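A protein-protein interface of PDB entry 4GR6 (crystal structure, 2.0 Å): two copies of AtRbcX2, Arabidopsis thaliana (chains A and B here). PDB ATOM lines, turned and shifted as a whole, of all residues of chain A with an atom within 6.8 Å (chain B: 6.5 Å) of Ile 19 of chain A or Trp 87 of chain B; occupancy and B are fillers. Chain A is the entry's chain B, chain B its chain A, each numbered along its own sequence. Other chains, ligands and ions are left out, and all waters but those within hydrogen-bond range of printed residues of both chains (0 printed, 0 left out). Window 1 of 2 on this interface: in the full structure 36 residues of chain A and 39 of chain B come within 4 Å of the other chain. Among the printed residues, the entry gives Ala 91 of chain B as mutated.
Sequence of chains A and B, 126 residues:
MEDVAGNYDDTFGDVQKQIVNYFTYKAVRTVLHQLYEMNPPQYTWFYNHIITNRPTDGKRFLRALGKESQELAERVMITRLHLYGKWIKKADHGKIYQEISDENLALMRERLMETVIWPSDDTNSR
Hydrophobic or aromatic side chains of chain B that line the printed part of chain A: Val 15, Ile 19, Tyr 22, Phe 23, Tyr 84, Trp 87, Ile 88, His 93 and Ile 96. Of the 16 printed residues of chain A, 12 touch a printed residue of chain B. Among the printed residues, 22 pairs touch across the chains. Among the printed residues, no Asp or Glu carboxylate lies within 4 Å of a Lys or Arg side-chain nitrogen of the other chain.
The side-chain hydroxyl (OH) of Tyr 84 of chain B sits at hydrogen-bond distance from a ring nitrogen (ND1) of His 93 of chain A (3.3 Å). The side-chain hydroxyl of Tyr 84 of chain A is in hydrogen-bond range of a ring nitrogen (ND1) of His 93 of chain B, 2.9 Å away. NE2 of His 93 of chain B sits at hydrogen-bond distance from NE2 of His 93 of chain A. OD2 of Asp 14 of chain A sits at hydrogen-bond distance from OH of Tyr 22 of chain B.
Printed residues of chain B within 4 Å of Phe 12 of chain A: Leu 83, Lys 86, Trp 87 and Lys 90. Ile 19 of chain A touches just one residue of chain B: Trp 87. Printed residues of chain B within 4 Å of Trp 87 of chain A: Val 15, Ile 19 and His 93. Printed residues of chain B within 4 Å of His 93 of chain A: Tyr 84, Ile 88 and His 93. Of the printed residues of chain A, Lys 86 of chain B touches Phe 12 (3.7 Å). Trp 87 of chain B touches just these residues of chain A: Phe 12 (3.6 Å), Val 15 (3.8 Å) and Ile 19 (3.7 Å). Of the printed residues of chain A, Lys 90 of chain B touches Phe 12 (3.5 Å). The nearest printed residue of chain A that does not touch Lys 90 of chain B is Val 15 of chain A (8.8 Å).
Val 15 of chain A touches Tyr 22 of chain B, and with the chains exchanged Tyr 22 of chain A touches Val 15 of chain B. Val 15 of chain A touches Phe 23 of chain B, and with the chains exchanged Phe 23 of chain A touches Val 15 of chain B. Val 15 of chain A touches Trp 87 of chain B, and with the chains exchanged Trp 87 of chain A touches Val 15 of chain B. Tyr 84 of chain A touches Ile 96 of chain B, and with the chains exchanged Ile 96 of chain A touches Tyr 84 of chain B. Positions printed for both chains: 15, 19, 22, 23, 84, 87, 93 and 96.
Among the printed residues, pairs that only touch across the chains: Phe 12 of chain A with Leu 83 of chain B, Phe 12 of chain A with Lys 86 of chain B, Phe 12 of chain A with Trp 87 of chain B, Phe 12 of chain A with Lys 90 of chain B, Val 15 of chain A with Tyr 22 of chain B, Val 15 of chain A with Phe 23 of chain B, Val 15 of chain A with Trp 87 of chain B, Gln 16 of chain A with Ile 96 of chain B, Gln 18 of chain A with Tyr 22 of chain B, Ile 19 of chain A with Trp 87 of chain B, Tyr 22 of chain A with Val 15 of chain B, Phe 23 of chain A with Val 15 of chain B, Tyr 84 of chain A with Ile 96 of chain B, Trp 87 of chain A with Val 15 of chain B, Trp 87 of chain A with Ile 19 of chain B, Trp 87 of chain A with His 93 of chain B, His 93 of chain A with Ile 88 of chain B and Ile 96 of chain A with Tyr 84 of chain B.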
ATOM      1  N   PHE A  12      25.766  23.013  -5.784  1.00  0.00           N
ATOM      2  CA  PHE A  12      26.653  21.941  -6.208  1.00  0.00           C
ATOM      3  C   PHE A  12      28.072  22.474  -6.559  1.00  0.00           C
ATOM      4  O   PHE A  12      28.866  21.793  -7.235  1.00  0.00           O
ATOM      5  CB  PHE A  12      26.029  21.205  -7.397  1.00  0.00           C
ATOM      6  CG  PHE A  12      24.704  20.524  -7.080  1.00  0.00           C
ATOM      7  CD1 PHE A  12      24.672  19.354  -6.337  1.00  0.00           C
ATOM      8  CD2 PHE A  12      23.511  21.044  -7.543  1.00  0.00           C
ATOM      9  CE1 PHE A  12      23.478  18.714  -6.054  1.00  0.00           C
ATOM     10  CE2 PHE A  12      22.288  20.409  -7.260  1.00  0.00           C
ATOM     11  CZ  PHE A  12      22.283  19.246  -6.510  1.00  0.00           C
ATOM     12  N   ASP A  14      30.402  22.693  -4.492  1.00  0.00           N
ATOM     13  CA  ASP A  14      31.273  21.707  -3.885  1.00  0.00           C
ATOM     14  C   ASP A  14      31.567  20.529  -4.835  1.00  0.00           C
ATOM     15  O   ASP A  14      32.695  19.985  -4.853  1.00  0.00           O
ATOM     16  CB  ASP A  14      30.664  21.230  -2.579  1.00  0.00           C
ATOM     17  CG  ASP A  14      29.230  20.666  -2.761  1.00  0.00           C
ATOM     18  OD1 ASP A  14      28.468  21.148  -3.625  1.00  0.00           O
ATOM     19  OD2 ASP A  14      28.857  19.754  -2.022  1.00  0.00           O
ATOM     20  N   VAL A  15      30.567  20.160  -5.639  1.00  0.00           N
ATOM     21  CA  VAL A  15      30.704  19.034  -6.569  1.00  0.00           C
ATOM     22  C   VAL A  15      31.648  19.332  -7.716  1.00  0.00           C
ATOM     23  O   VAL A  15      32.429  18.484  -8.101  1.00  0.00           O
ATOM     24  CB  VAL A  15      29.340  18.661  -7.204  1.00  0.00           C
ATOM     25  CG1 VAL A  15      29.507  17.558  -8.246  1.00  0.00           C
ATOM     26  CG2 VAL A  15      28.348  18.233  -6.114  1.00  0.00           C
ATOM     27  N   GLN A  16      31.484  20.506  -8.314  1.00  0.00           N
ATOM     28  CA  GLN A  16      32.316  20.917  -9.394  1.00  0.00           C
ATOM     29  C   GLN A  16      33.773  20.910  -8.906  1.00  0.00           C
ATOM     30  O   GLN A  16      34.675  20.456  -9.613  1.00  0.00           O
ATOM     31  CB  GLN A  16      31.917  22.311  -9.854  1.00  0.00           C
ATOM     32  CG  GLN A  16      32.813  22.845 -10.975  1.00  0.00           C
ATOM     33  CD  GLN A  16      32.432  24.245 -11.432  1.00  0.00           C
ATOM     34  OE1 GLN A  16      31.510  24.861 -10.895  1.00  0.00           O
ATOM     35  NE2 GLN A  16      33.143  24.751 -12.432  1.00  0.00           N
ATOM     36  N   LYS A  17      33.991  21.386  -7.686  1.00  0.00           N
ATOM     37  CA  LYS A  17      35.354  21.538  -7.170  1.00  0.00           C
ATOM     38  C   LYS A  17      35.949  20.167  -6.895  1.00  0.00           C
ATOM     39  O   LYS A  17      37.085  19.896  -7.261  1.00  0.00           O
ATOM     40  CB  LYS A  17      35.388  22.425  -5.915  1.00  0.00           C
ATOM     41  N   GLN A  18      35.180  19.281  -6.280  1.00  0.00           N
ATOM     42  CA  GLN A  18      35.694  17.965  -5.967  1.00  0.00           C
ATOM     43  C   GLN A  18      36.040  17.197  -7.248  1.00  0.00           C
ATOM     44  O   GLN A  18      36.946  16.369  -7.240  1.00  0.00           O
ATOM     45  CB  GLN A  18      34.675  17.170  -5.149  1.00  0.00           C
ATOM     46  CG  GLN A  18      35.246  15.919  -4.478  1.00  0.00           C
ATOM     47  N   ILE A  19      35.288  17.441  -8.322  1.00  0.00           N
ATOM     48  CA  ILE A  19      35.492  16.721  -9.558  1.00  0.00           C
ATOM     49  C   ILE A  19      36.778  17.216 -10.227  1.00  0.00           C
ATOM     50  O   ILE A  19      37.533  16.423 -10.758  1.00  0.00           O
ATOM     51  CB  ILE A  19      34.316  16.891 -10.516  1.00  0.00           C
ATOM     52  CG1 ILE A  19      33.140  16.002 -10.081  1.00  0.00           C
ATOM     53  CG2 ILE A  19      34.719  16.491 -11.912  1.00  0.00           C
ATOM     54  CD1 ILE A  19      31.825  16.289 -10.834  1.00  0.00           C
ATOM     55  N   VAL A  20      36.995  18.521 -10.174  1.00  0.00           N
ATOM     56  CA  VAL A  20      38.189  19.131 -10.707  1.00  0.00           C
ATOM     57  C   VAL A  20      39.395  18.694  -9.897  1.00  0.00           C
ATOM     58  O   VAL A  20      40.431  18.397 -10.464  1.00  0.00           O
ATOM     59  CB  VAL A  20      38.072  20.649 -10.735  1.00  0.00           C
ATOM     60  CG1 VAL A  20      39.387  21.283 -11.135  1.00  0.00           C
ATOM     61  CG2 VAL A  20      36.969  21.066 -11.723  1.00  0.00           C
ATOM     62  N   ASN A  21      39.253  18.635  -8.577  1.00  0.00           N
ATOM     63  CA  ASN A  21      40.293  18.082  -7.728  1.00  0.00           C
ATOM     64  C   ASN A  21      40.646  16.675  -8.130  1.00  0.00           C
ATOM     65  O   ASN A  21      41.818  16.330  -8.202  1.00  0.00           O
ATOM     66  CB  ASN A  21      39.876  18.081  -6.253  1.00  0.00           C
ATOM     67  CG  ASN A  21      39.847  19.460  -5.666  1.00  0.00           C
ATOM     68  OD1 ASN A  21      40.298  20.427  -6.287  1.00  0.00           O
ATOM     69  ND2 ASN A  21      39.317  19.572  -4.452  1.00  0.00           N
ATOM     70  N   TYR A  22      39.633  15.849  -8.381  1.00  0.00           N
ATOM     71  CA  TYR A  22      39.890  14.454  -8.741  1.00  0.00           C
ATOM     72  C   TYR A  22      40.638  14.315 -10.082  1.00  0.00           C
ATOM     73  O   TYR A  22      41.513  13.451 -10.208  1.00  0.00           O
ATOM     74  CB  TYR A  22      38.573  13.599  -8.787  1.00  0.00           C
ATOM     75  CG  TYR A  22      38.890  12.140  -9.069  1.00  0.00           C
ATOM     76  CD1 TYR A  22      39.523  11.356  -8.116  1.00  0.00           C
ATOM     77  CD2 TYR A  22      38.593  11.559 -10.292  1.00  0.00           C
ATOM     78  CE1 TYR A  22      39.861  10.031  -8.382  1.00  0.00           C
ATOM     79  CE2 TYR A  22      38.910  10.236 -10.559  1.00  0.00           C
ATOM     80  CZ  TYR A  22      39.556   9.482  -9.599  1.00  0.00           C
ATOM     81  OH  TYR A  22      39.892   8.175  -9.852  1.00  0.00           O
ATOM     82  N   PHE A  23      40.254  15.123 -11.077  1.00  0.00           N
ATOM     83  CA  PHE A  23      40.883  15.095 -12.391  1.00  0.00           C
ATOM     84  C   PHE A  23      42.342  15.657 -12.287  1.00  0.00           C
ATOM     85  O   PHE A  23      43.244  15.232 -13.010  1.00  0.00           O
ATOM     86  CB  PHE A  23      40.050  15.891 -13.381  1.00  0.00           C
ATOM     87  CG  PHE A  23      38.994  15.049 -14.089  1.00  0.00           C
ATOM     88  CD1 PHE A  23      39.287  14.395 -15.263  1.00  0.00           C
ATOM     89  CD2 PHE A  23      37.757  14.867 -13.527  1.00  0.00           C
ATOM     90  CE1 PHE A  23      38.334  13.590 -15.910  1.00  0.00           C
ATOM     91  CE2 PHE A  23      36.792  14.070 -14.169  1.00  0.00           C
ATOM     92  CZ  PHE A  23      37.101  13.429 -15.349  1.00  0.00           C
ATOM     93  N   THR A  24      42.544  16.560 -11.346  1.00  0.00           N
ATOM     94  CA  THR A  24      43.898  17.074 -11.084  1.00  0.00           C
ATOM     95  C   THR A  24      44.730  15.927 -10.543  1.00  0.00           C
ATOM     96  O   THR A  24      45.854  15.664 -11.013  1.00  0.00           O
ATOM     97  CB  THR A  24      43.892  18.284 -10.149  1.00  0.00           C
ATOM     98  OG1 THR A  24      43.070  19.315 -10.701  1.00  0.00           O
ATOM     99  CG2 THR A  24      45.332  18.872  -9.997  1.00  0.00           C
ATOM    100  N   TYR A  84      39.583  15.620 -18.623  1.00  0.00           N
ATOM    101  CA  TYR A  84      38.217  16.068 -18.379  1.00  0.00           C
ATOM    102  C   TYR A  84      37.430  16.100 -19.686  1.00  0.00           C
ATOM    103  O   TYR A  84      36.286  15.657 -19.732  1.00  0.00           O
ATOM    104  CB  TYR A  84      38.165  17.416 -17.664  1.00  0.00           C
ATOM    105  CG  TYR A  84      36.756  17.745 -17.214  1.00  0.00           C
ATOM    106  CD1 TYR A  84      36.189  17.112 -16.106  1.00  0.00           C
ATOM    107  CD2 TYR A  84      35.987  18.648 -17.910  1.00  0.00           C
ATOM    108  CE1 TYR A  84      34.869  17.379 -15.726  1.00  0.00           C
ATOM    109  CE2 TYR A  84      34.682  18.921 -17.535  1.00  0.00           C
ATOM    110  CZ  TYR A  84      34.138  18.289 -16.438  1.00  0.00           C
ATOM    111  OH  TYR A  84      32.848  18.585 -16.066  1.00  0.00           O
ATOM    112  N   TRP A  87      36.455  12.581 -20.728  1.00  0.00           N
ATOM    113  CA  TRP A  87      35.372  12.050 -19.902  1.00  0.00           C
ATOM    114  C   TRP A  87      34.012  12.584 -20.360  1.00  0.00           C
ATOM    115  O   TRP A  87      33.062  11.803 -20.561  1.00  0.00           O
ATOM    116  CB  TRP A  87      35.596  12.356 -18.419  1.00  0.00           C
ATOM    117  CG  TRP A  87      34.420  11.952 -17.521  1.00  0.00           C
ATOM    118  CD1 TRP A  87      33.958  10.681 -17.262  1.00  0.00           C
ATOM    119  CD2 TRP A  87      33.593  12.834 -16.770  1.00  0.00           C
ATOM    120  NE1 TRP A  87      32.891  10.735 -16.395  1.00  0.00           N
ATOM    121  CE2 TRP A  87      32.642  12.047 -16.085  1.00  0.00           C
ATOM    122  CE3 TRP A  87      33.552  14.217 -16.620  1.00  0.00           C
ATOM    123  CZ2 TRP A  87      31.688  12.598 -15.252  1.00  0.00           C
ATOM    124  CZ3 TRP A  87      32.582  14.769 -15.787  1.00  0.00           C
ATOM    125  CH2 TRP A  87      31.673  13.961 -15.111  1.00  0.00           C
ATOM    126  N   HIS A  93      25.358  10.432 -17.905  1.00  0.00           N
ATOM    127  CA  HIS A  93      24.933  10.743 -16.563  1.00  0.00           C
ATOM    128  C   HIS A  93      23.626  10.052 -16.201  1.00  0.00           C
ATOM    129  O   HIS A  93      23.436   9.654 -15.060  1.00  0.00           O
ATOM    130  CB  HIS A  93      24.866  12.265 -16.409  1.00  0.00           C
ATOM    131  CG  HIS A  93      26.189  12.928 -16.623  1.00  0.00           C
ATOM    132  ND1 HIS A  93      27.172  12.946 -15.653  1.00  0.00           N
ATOM    133  CD2 HIS A  93      26.713  13.555 -17.702  1.00  0.00           C
ATOM    134  CE1 HIS A  93      28.240  13.564 -16.125  1.00  0.00           C
ATOM    135  NE2 HIS A  93      27.989  13.937 -17.368  1.00  0.00           N
ATOM    136  N   ILE A  96      24.567   6.731 -14.997  1.00  0.00           N
ATOM    137  CA  ILE A  96      25.095   6.769 -13.638  1.00  0.00           C
ATOM    138  C   ILE A  96      23.961   6.878 -12.616  1.00  0.00           C
ATOM    139  O   ILE A  96      23.979   6.215 -11.585  1.00  0.00           O
ATOM    140  CB  ILE A  96      26.082   7.936 -13.436  1.00  0.00           C
ATOM    141  CG1 ILE A  96      27.284   7.768 -14.384  1.00  0.00           C
ATOM    142  CG2 ILE A  96      26.544   7.983 -11.985  1.00  0.00           C
ATOM    143  CD1 ILE A  96      28.267   8.953 -14.367  1.00  0.00           C
ATOM    144  N   VAL B  15      36.129   7.320 -12.366  1.00  0.00           N
ATOM    145  CA  VAL B  15      35.515   8.633 -12.237  1.00  0.00           C
ATOM    146  C   VAL B  15      34.087   8.445 -11.726  1.00  0.00           C
ATOM    147  O   VAL B  15      33.653   9.131 -10.805  1.00  0.00           O
ATOM    148  CB  VAL B  15      35.528   9.416 -13.574  1.00  0.00           C
ATOM    149  CG1 VAL B  15      34.683  10.693 -13.470  1.00  0.00           C
ATOM    150  CG2 VAL B  15      36.992   9.782 -13.957  1.00  0.00           C
ATOM    151  N   ILE B  19      32.532   9.979  -8.215  1.00  0.00           N
ATOM    152  CA  ILE B  19      31.358  10.835  -8.255  1.00  0.00           C
ATOM    153  C   ILE B  19      30.300  10.260  -7.311  1.00  0.00           C
ATOM    154  O   ILE B  19      29.736  10.967  -6.500  1.00  0.00           O
ATOM    155  CB  ILE B  19      30.797  10.929  -9.683  1.00  0.00           C
ATOM    156  CG1 ILE B  19      31.644  11.903 -10.520  1.00  0.00           C
ATOM    157  CG2 ILE B  19      29.335  11.352  -9.645  1.00  0.00           C
ATOM    158  CD1 ILE B  19      31.336  11.894 -12.027  1.00  0.00           C
ATOM    159  N   TYR B  22      31.291  10.854  -3.791  1.00  0.00           N
ATOM    160  CA  TYR B  22      31.101  12.202  -3.360  1.00  0.00           C
ATOM    161  C   TYR B  22      29.605  12.496  -3.110  1.00  0.00           C
ATOM    162  O   TYR B  22      29.299  13.179  -2.161  1.00  0.00           O
ATOM    163  CB  TYR B  22      31.658  13.232  -4.340  1.00  0.00           C
ATOM    164  CG  TYR B  22      31.539  14.607  -3.745  1.00  0.00           C
ATOM    165  CD1 TYR B  22      32.333  14.975  -2.661  1.00  0.00           C
ATOM    166  CD2 TYR B  22      30.597  15.523  -4.214  1.00  0.00           C
ATOM    167  CE1 TYR B  22      32.215  16.202  -2.078  1.00  0.00           C
ATOM    168  CE2 TYR B  22      30.469  16.772  -3.623  1.00  0.00           C
ATOM    169  CZ  TYR B  22      31.279  17.100  -2.550  1.00  0.00           C
ATOM    170  OH  TYR B  22      31.167  18.338  -1.949  1.00  0.00           O
ATOM    171  N   PHE B  23      28.688  12.021  -3.964  1.00  0.00           N
ATOM    172  CA  PHE B  23      27.275  12.298  -3.682  1.00  0.00           C
ATOM    173  C   PHE B  23      26.812  11.577  -2.424  1.00  0.00           C
ATOM    174  O   PHE B  23      25.906  12.047  -1.722  1.00  0.00           O
ATOM    175  CB  PHE B  23      26.382  12.023  -4.903  1.00  0.00           C
ATOM    176  CG  PHE B  23      26.366  13.176  -5.878  1.00  0.00           C
ATOM    177  CD1 PHE B  23      27.375  13.331  -6.806  1.00  0.00           C
ATOM    178  CD2 PHE B  23      25.391  14.136  -5.817  1.00  0.00           C
ATOM    179  CE1 PHE B  23      27.399  14.401  -7.664  1.00  0.00           C
ATOM    180  CE2 PHE B  23      25.377  15.216  -6.714  1.00  0.00           C
ATOM    181  CZ  PHE B  23      26.404  15.363  -7.617  1.00  0.00           C
ATOM    182  N   HIS B  82      18.587  11.527  -5.191  1.00  0.00           N
ATOM    183  CA  HIS B  82      17.873  12.764  -5.558  1.00  0.00           C
ATOM    184  C   HIS B  82      18.811  13.941  -5.783  1.00  0.00           C
ATOM    185  O   HIS B  82      18.578  14.752  -6.681  1.00  0.00           O
ATOM    186  CB  HIS B  82      16.840  13.123  -4.501  1.00  0.00           C
ATOM    187  CG  HIS B  82      15.721  12.135  -4.433  1.00  0.00           C
ATOM    188  ND1 HIS B  82      14.592  12.352  -3.693  1.00  0.00           N
ATOM    189  CD2 HIS B  82      15.579  10.905  -4.997  1.00  0.00           C
ATOM    190  CE1 HIS B  82      13.767  11.321  -3.830  1.00  0.00           C
ATOM    191  NE2 HIS B  82      14.340  10.428  -4.615  1.00  0.00           N
ATOM    192  N   LEU B  83      19.848  14.042  -4.961  1.00  0.00           N
ATOM    193  CA  LEU B  83      20.896  15.062  -5.208  1.00  0.00           C
ATOM    194  C   LEU B  83      21.556  14.896  -6.572  1.00  0.00           C
ATOM    195  O   LEU B  83      21.766  15.870  -7.287  1.00  0.00           O
ATOM    196  CB  LEU B  83      21.989  14.984  -4.137  1.00  0.00           C
ATOM    197  CG  LEU B  83      21.580  15.532  -2.773  1.00  0.00           C
ATOM    198  CD1 LEU B  83      22.702  15.183  -1.793  1.00  0.00           C
ATOM    199  CD2 LEU B  83      21.243  17.064  -2.821  1.00  0.00           C
ATOM    200  N   TYR B  84      21.940  13.664  -6.916  1.00  0.00           N
ATOM    201  CA  TYR B  84      22.510  13.413  -8.243  1.00  0.00           C
ATOM    202  C   TYR B  84      21.559  13.826  -9.348  1.00  0.00           C
ATOM    203  O   TYR B  84      21.961  14.472 -10.328  1.00  0.00           O
ATOM    204  CB  TYR B  84      22.915  11.944  -8.388  1.00  0.00           C
ATOM    205  CG  TYR B  84      23.804  11.745  -9.594  1.00  0.00           C
ATOM    206  CD1 TYR B  84      25.154  12.130  -9.549  1.00  0.00           C
ATOM    207  CD2 TYR B  84      23.313  11.228 -10.774  1.00  0.00           C
ATOM    208  CE1 TYR B  84      25.983  11.973 -10.653  1.00  0.00           C
ATOM    209  CE2 TYR B  84      24.146  11.081 -11.901  1.00  0.00           C
ATOM    210  CZ  TYR B  84      25.477  11.458 -11.816  1.00  0.00           C
ATOM    211  OH  TYR B  84      26.313  11.321 -12.890  1.00  0.00           O
ATOM    212  N   GLY B  85      20.289  13.451  -9.198  1.00  0.00           N
ATOM    213  CA  GLY B  85      19.261  13.907 -10.125  1.00  0.00           C
ATOM    214  C   GLY B  85      19.191  15.419 -10.315  1.00  0.00           C
ATOM    215  O   GLY B  85      19.092  15.905 -11.437  1.00  0.00           O
ATOM    216  N   LYS B  86      19.225  16.174  -9.221  1.00  0.00           N
ATOM    217  CA  LYS B  86      19.145  17.631  -9.322  1.00  0.00           C
ATOM    218  C   LYS B  86      20.387  18.169  -9.992  1.00  0.00           C
ATOM    219  O   LYS B  86      20.329  19.117 -10.792  1.00  0.00           O
ATOM    220  CB  LYS B  86      19.015  18.259  -7.920  1.00  0.00           C
ATOM    221  CG  LYS B  86      17.677  17.946  -7.275  1.00  0.00           C
ATOM    222  CD  LYS B  86      17.616  18.373  -5.812  1.00  0.00           C
ATOM    223  CE  LYS B  86      16.297  17.948  -5.169  1.00  0.00           C
ATOM    224  NZ  LYS B  86      16.130  18.488  -3.789  1.00  0.00           N
ATOM    225  N   TRP B  87      21.534  17.576  -9.641  1.00  0.00           N
ATOM    226  CA  TRP B  87      22.790  18.000 -10.234  1.00  0.00           C
ATOM    227  C   TRP B  87      22.814  17.810 -11.738  1.00  0.00           C
ATOM    228  O   TRP B  87      23.176  18.710 -12.494  1.00  0.00           O
ATOM    229  CB  TRP B  87      23.983  17.220  -9.632  1.00  0.00           C
ATOM    230  CG  TRP B  87      25.305  17.645 -10.270  1.00  0.00           C
ATOM    231  CD1 TRP B  87      25.825  18.921 -10.313  1.00  0.00           C
ATOM    232  CD2 TRP B  87      26.255  16.814 -10.947  1.00  0.00           C
ATOM    233  NE1 TRP B  87      27.005  18.923 -10.968  1.00  0.00           N
ATOM    234  CE2 TRP B  87      27.309  17.647 -11.365  1.00  0.00           C
ATOM    235  CE3 TRP B  87      26.322  15.451 -11.225  1.00  0.00           C
ATOM    236  CZ2 TRP B  87      28.433  17.161 -12.052  1.00  0.00           C
ATOM    237  CZ3 TRP B  87      27.442  14.958 -11.909  1.00  0.00           C
ATOM    238  CH2 TRP B  87      28.476  15.816 -12.325  1.00  0.00           C
ATOM    239  N   ILE B  88      22.487  16.614 -12.195  1.00  0.00           N
ATOM    240  CA  ILE B  88      22.611  16.378 -13.617  1.00  0.00           C
ATOM    241  C   ILE B  88      21.611  17.202 -14.413  1.00  0.00           C
ATOM    242  O   ILE B  88      21.826  17.436 -15.594  1.00  0.00           O
ATOM    243  CB  ILE B  88      22.537  14.884 -14.000  1.00  0.00           C
ATOM    244  CG1 ILE B  88      21.188  14.276 -13.616  1.00  0.00           C
ATOM    245  CG2 ILE B  88      23.730  14.153 -13.354  1.00  0.00           C
ATOM    246  CD1 ILE B  88      21.102  12.817 -13.962  1.00  0.00           C
ATOM    247  N   LYS B  89      20.564  17.694 -13.773  1.00  0.00           N
ATOM    248  CA  LYS B  89      19.560  18.453 -14.516  1.00  0.00           C
ATOM    249  C   LYS B  89      20.093  19.817 -14.893  1.00  0.00           C
ATOM    250  O   LYS B  89      19.631  20.413 -15.858  1.00  0.00           O
ATOM    251  CB  LYS B  89      18.262  18.628 -13.708  1.00  0.00           C
ATOM    252  CG  LYS B  89      17.221  17.569 -13.956  1.00  0.00           C
ATOM    253  CD  LYS B  89      15.812  18.106 -13.685  1.00  0.00           C
ATOM    254  N   LYS B  90      21.073  20.320 -14.147  1.00  0.00           N
ATOM    255  CA  LYS B  90      21.577  21.659 -14.419  1.00  0.00           C
ATOM    256  C   LYS B  90      23.059  21.725 -14.736  1.00  0.00           C
ATOM    257  O   LYS B  90      23.521  22.747 -15.207  1.00  0.00           O
ATOM    258  CB  LYS B  90      21.258  22.599 -13.254  1.00  0.00           C
ATOM    259  CG  LYS B  90      22.017  22.327 -11.979  1.00  0.00           C
ATOM    260  CD  LYS B  90      21.331  23.017 -10.806  1.00  0.00           C
ATOM    261  CE  LYS B  90      22.341  23.495  -9.781  1.00  0.00           C
ATOM    262  NZ  LYS B  90      21.706  23.936  -8.499  1.00  0.00           N
ATOM    263  N   ALA B  91      23.807  20.653 -14.472  1.00  0.00           N
ATOM    264  CA  ALA B  91      25.249  20.687 -14.693  1.00  0.00           C
ATOM    265  C   ALA B  91      25.553  21.041 -16.139  1.00  0.00           C
ATOM    266  O   ALA B  91      24.935  20.518 -17.073  1.00  0.00           O
ATOM    267  CB  ALA B  91      25.895  19.349 -14.324  1.00  0.00           C
ATOM    268  N   ASP B  92      26.492  21.953 -16.312  1.00  0.00           N
ATOM    269  CA  ASP B  92      26.928  22.374 -17.629  1.00  0.00           C
ATOM    270  C   ASP B  92      28.399  21.998 -17.772  1.00  0.00           C
ATOM    271  O   ASP B  92      29.284  22.750 -17.347  1.00  0.00           O
ATOM    272  CB  ASP B  92      26.752  23.885 -17.759  1.00  0.00           C
ATOM    273  CG  ASP B  92      27.120  24.402 -19.127  1.00  0.00           C
ATOM    274  OD1 ASP B  92      27.825  23.688 -19.890  1.00  0.00           O
ATOM    275  OD2 ASP B  92      26.685  25.535 -19.444  1.00  0.00           O
ATOM    276  N   HIS B  93      28.667  20.847 -18.376  1.00  0.00           N
ATOM    277  CA  HIS B  93      30.026  20.294 -18.354  1.00  0.00           C
ATOM    278  C   HIS B  93      30.955  21.011 -19.308  1.00  0.00           C
ATOM    279  O   HIS B  93      32.163  21.043 -19.095  1.00  0.00           O
ATOM    280  CB  HIS B  93      29.994  18.786 -18.609  1.00  0.00           C
ATOM    281  CG  HIS B  93      29.384  18.029 -17.476  1.00  0.00           C
ATOM    282  ND1 HIS B  93      30.067  17.786 -16.302  1.00  0.00           N
ATOM    283  CD2 HIS B  93      28.137  17.531 -17.302  1.00  0.00           C
ATOM    284  CE1 HIS B  93      29.275  17.137 -15.467  1.00  0.00           C
ATOM    285  NE2 HIS B  93      28.099  16.974 -16.048  1.00  0.00           N
ATOM    286  N   ILE B  96      32.262  23.743 -17.185  1.00  0.00           N
ATOM    287  CA  ILE B  96      33.301  23.328 -16.257  1.00  0.00           C
ATOM    288  C   ILE B  96      34.633  23.194 -16.993  1.00  0.00           C
ATOM    289  O   ILE B  96      35.650  23.608 -16.485  1.00  0.00           O
ATOM    290  CB  ILE B  96      32.949  22.016 -15.568  1.00  0.00           C
ATOM    291  CG1 ILE B  96      31.676  22.203 -14.736  1.00  0.00           C
ATOM    292  CG2 ILE B  96      34.124  21.573 -14.687  1.00  0.00           C
ATOM    293  CD1 ILE B  96      31.110  20.918 -14.169  1.00  0.00           C
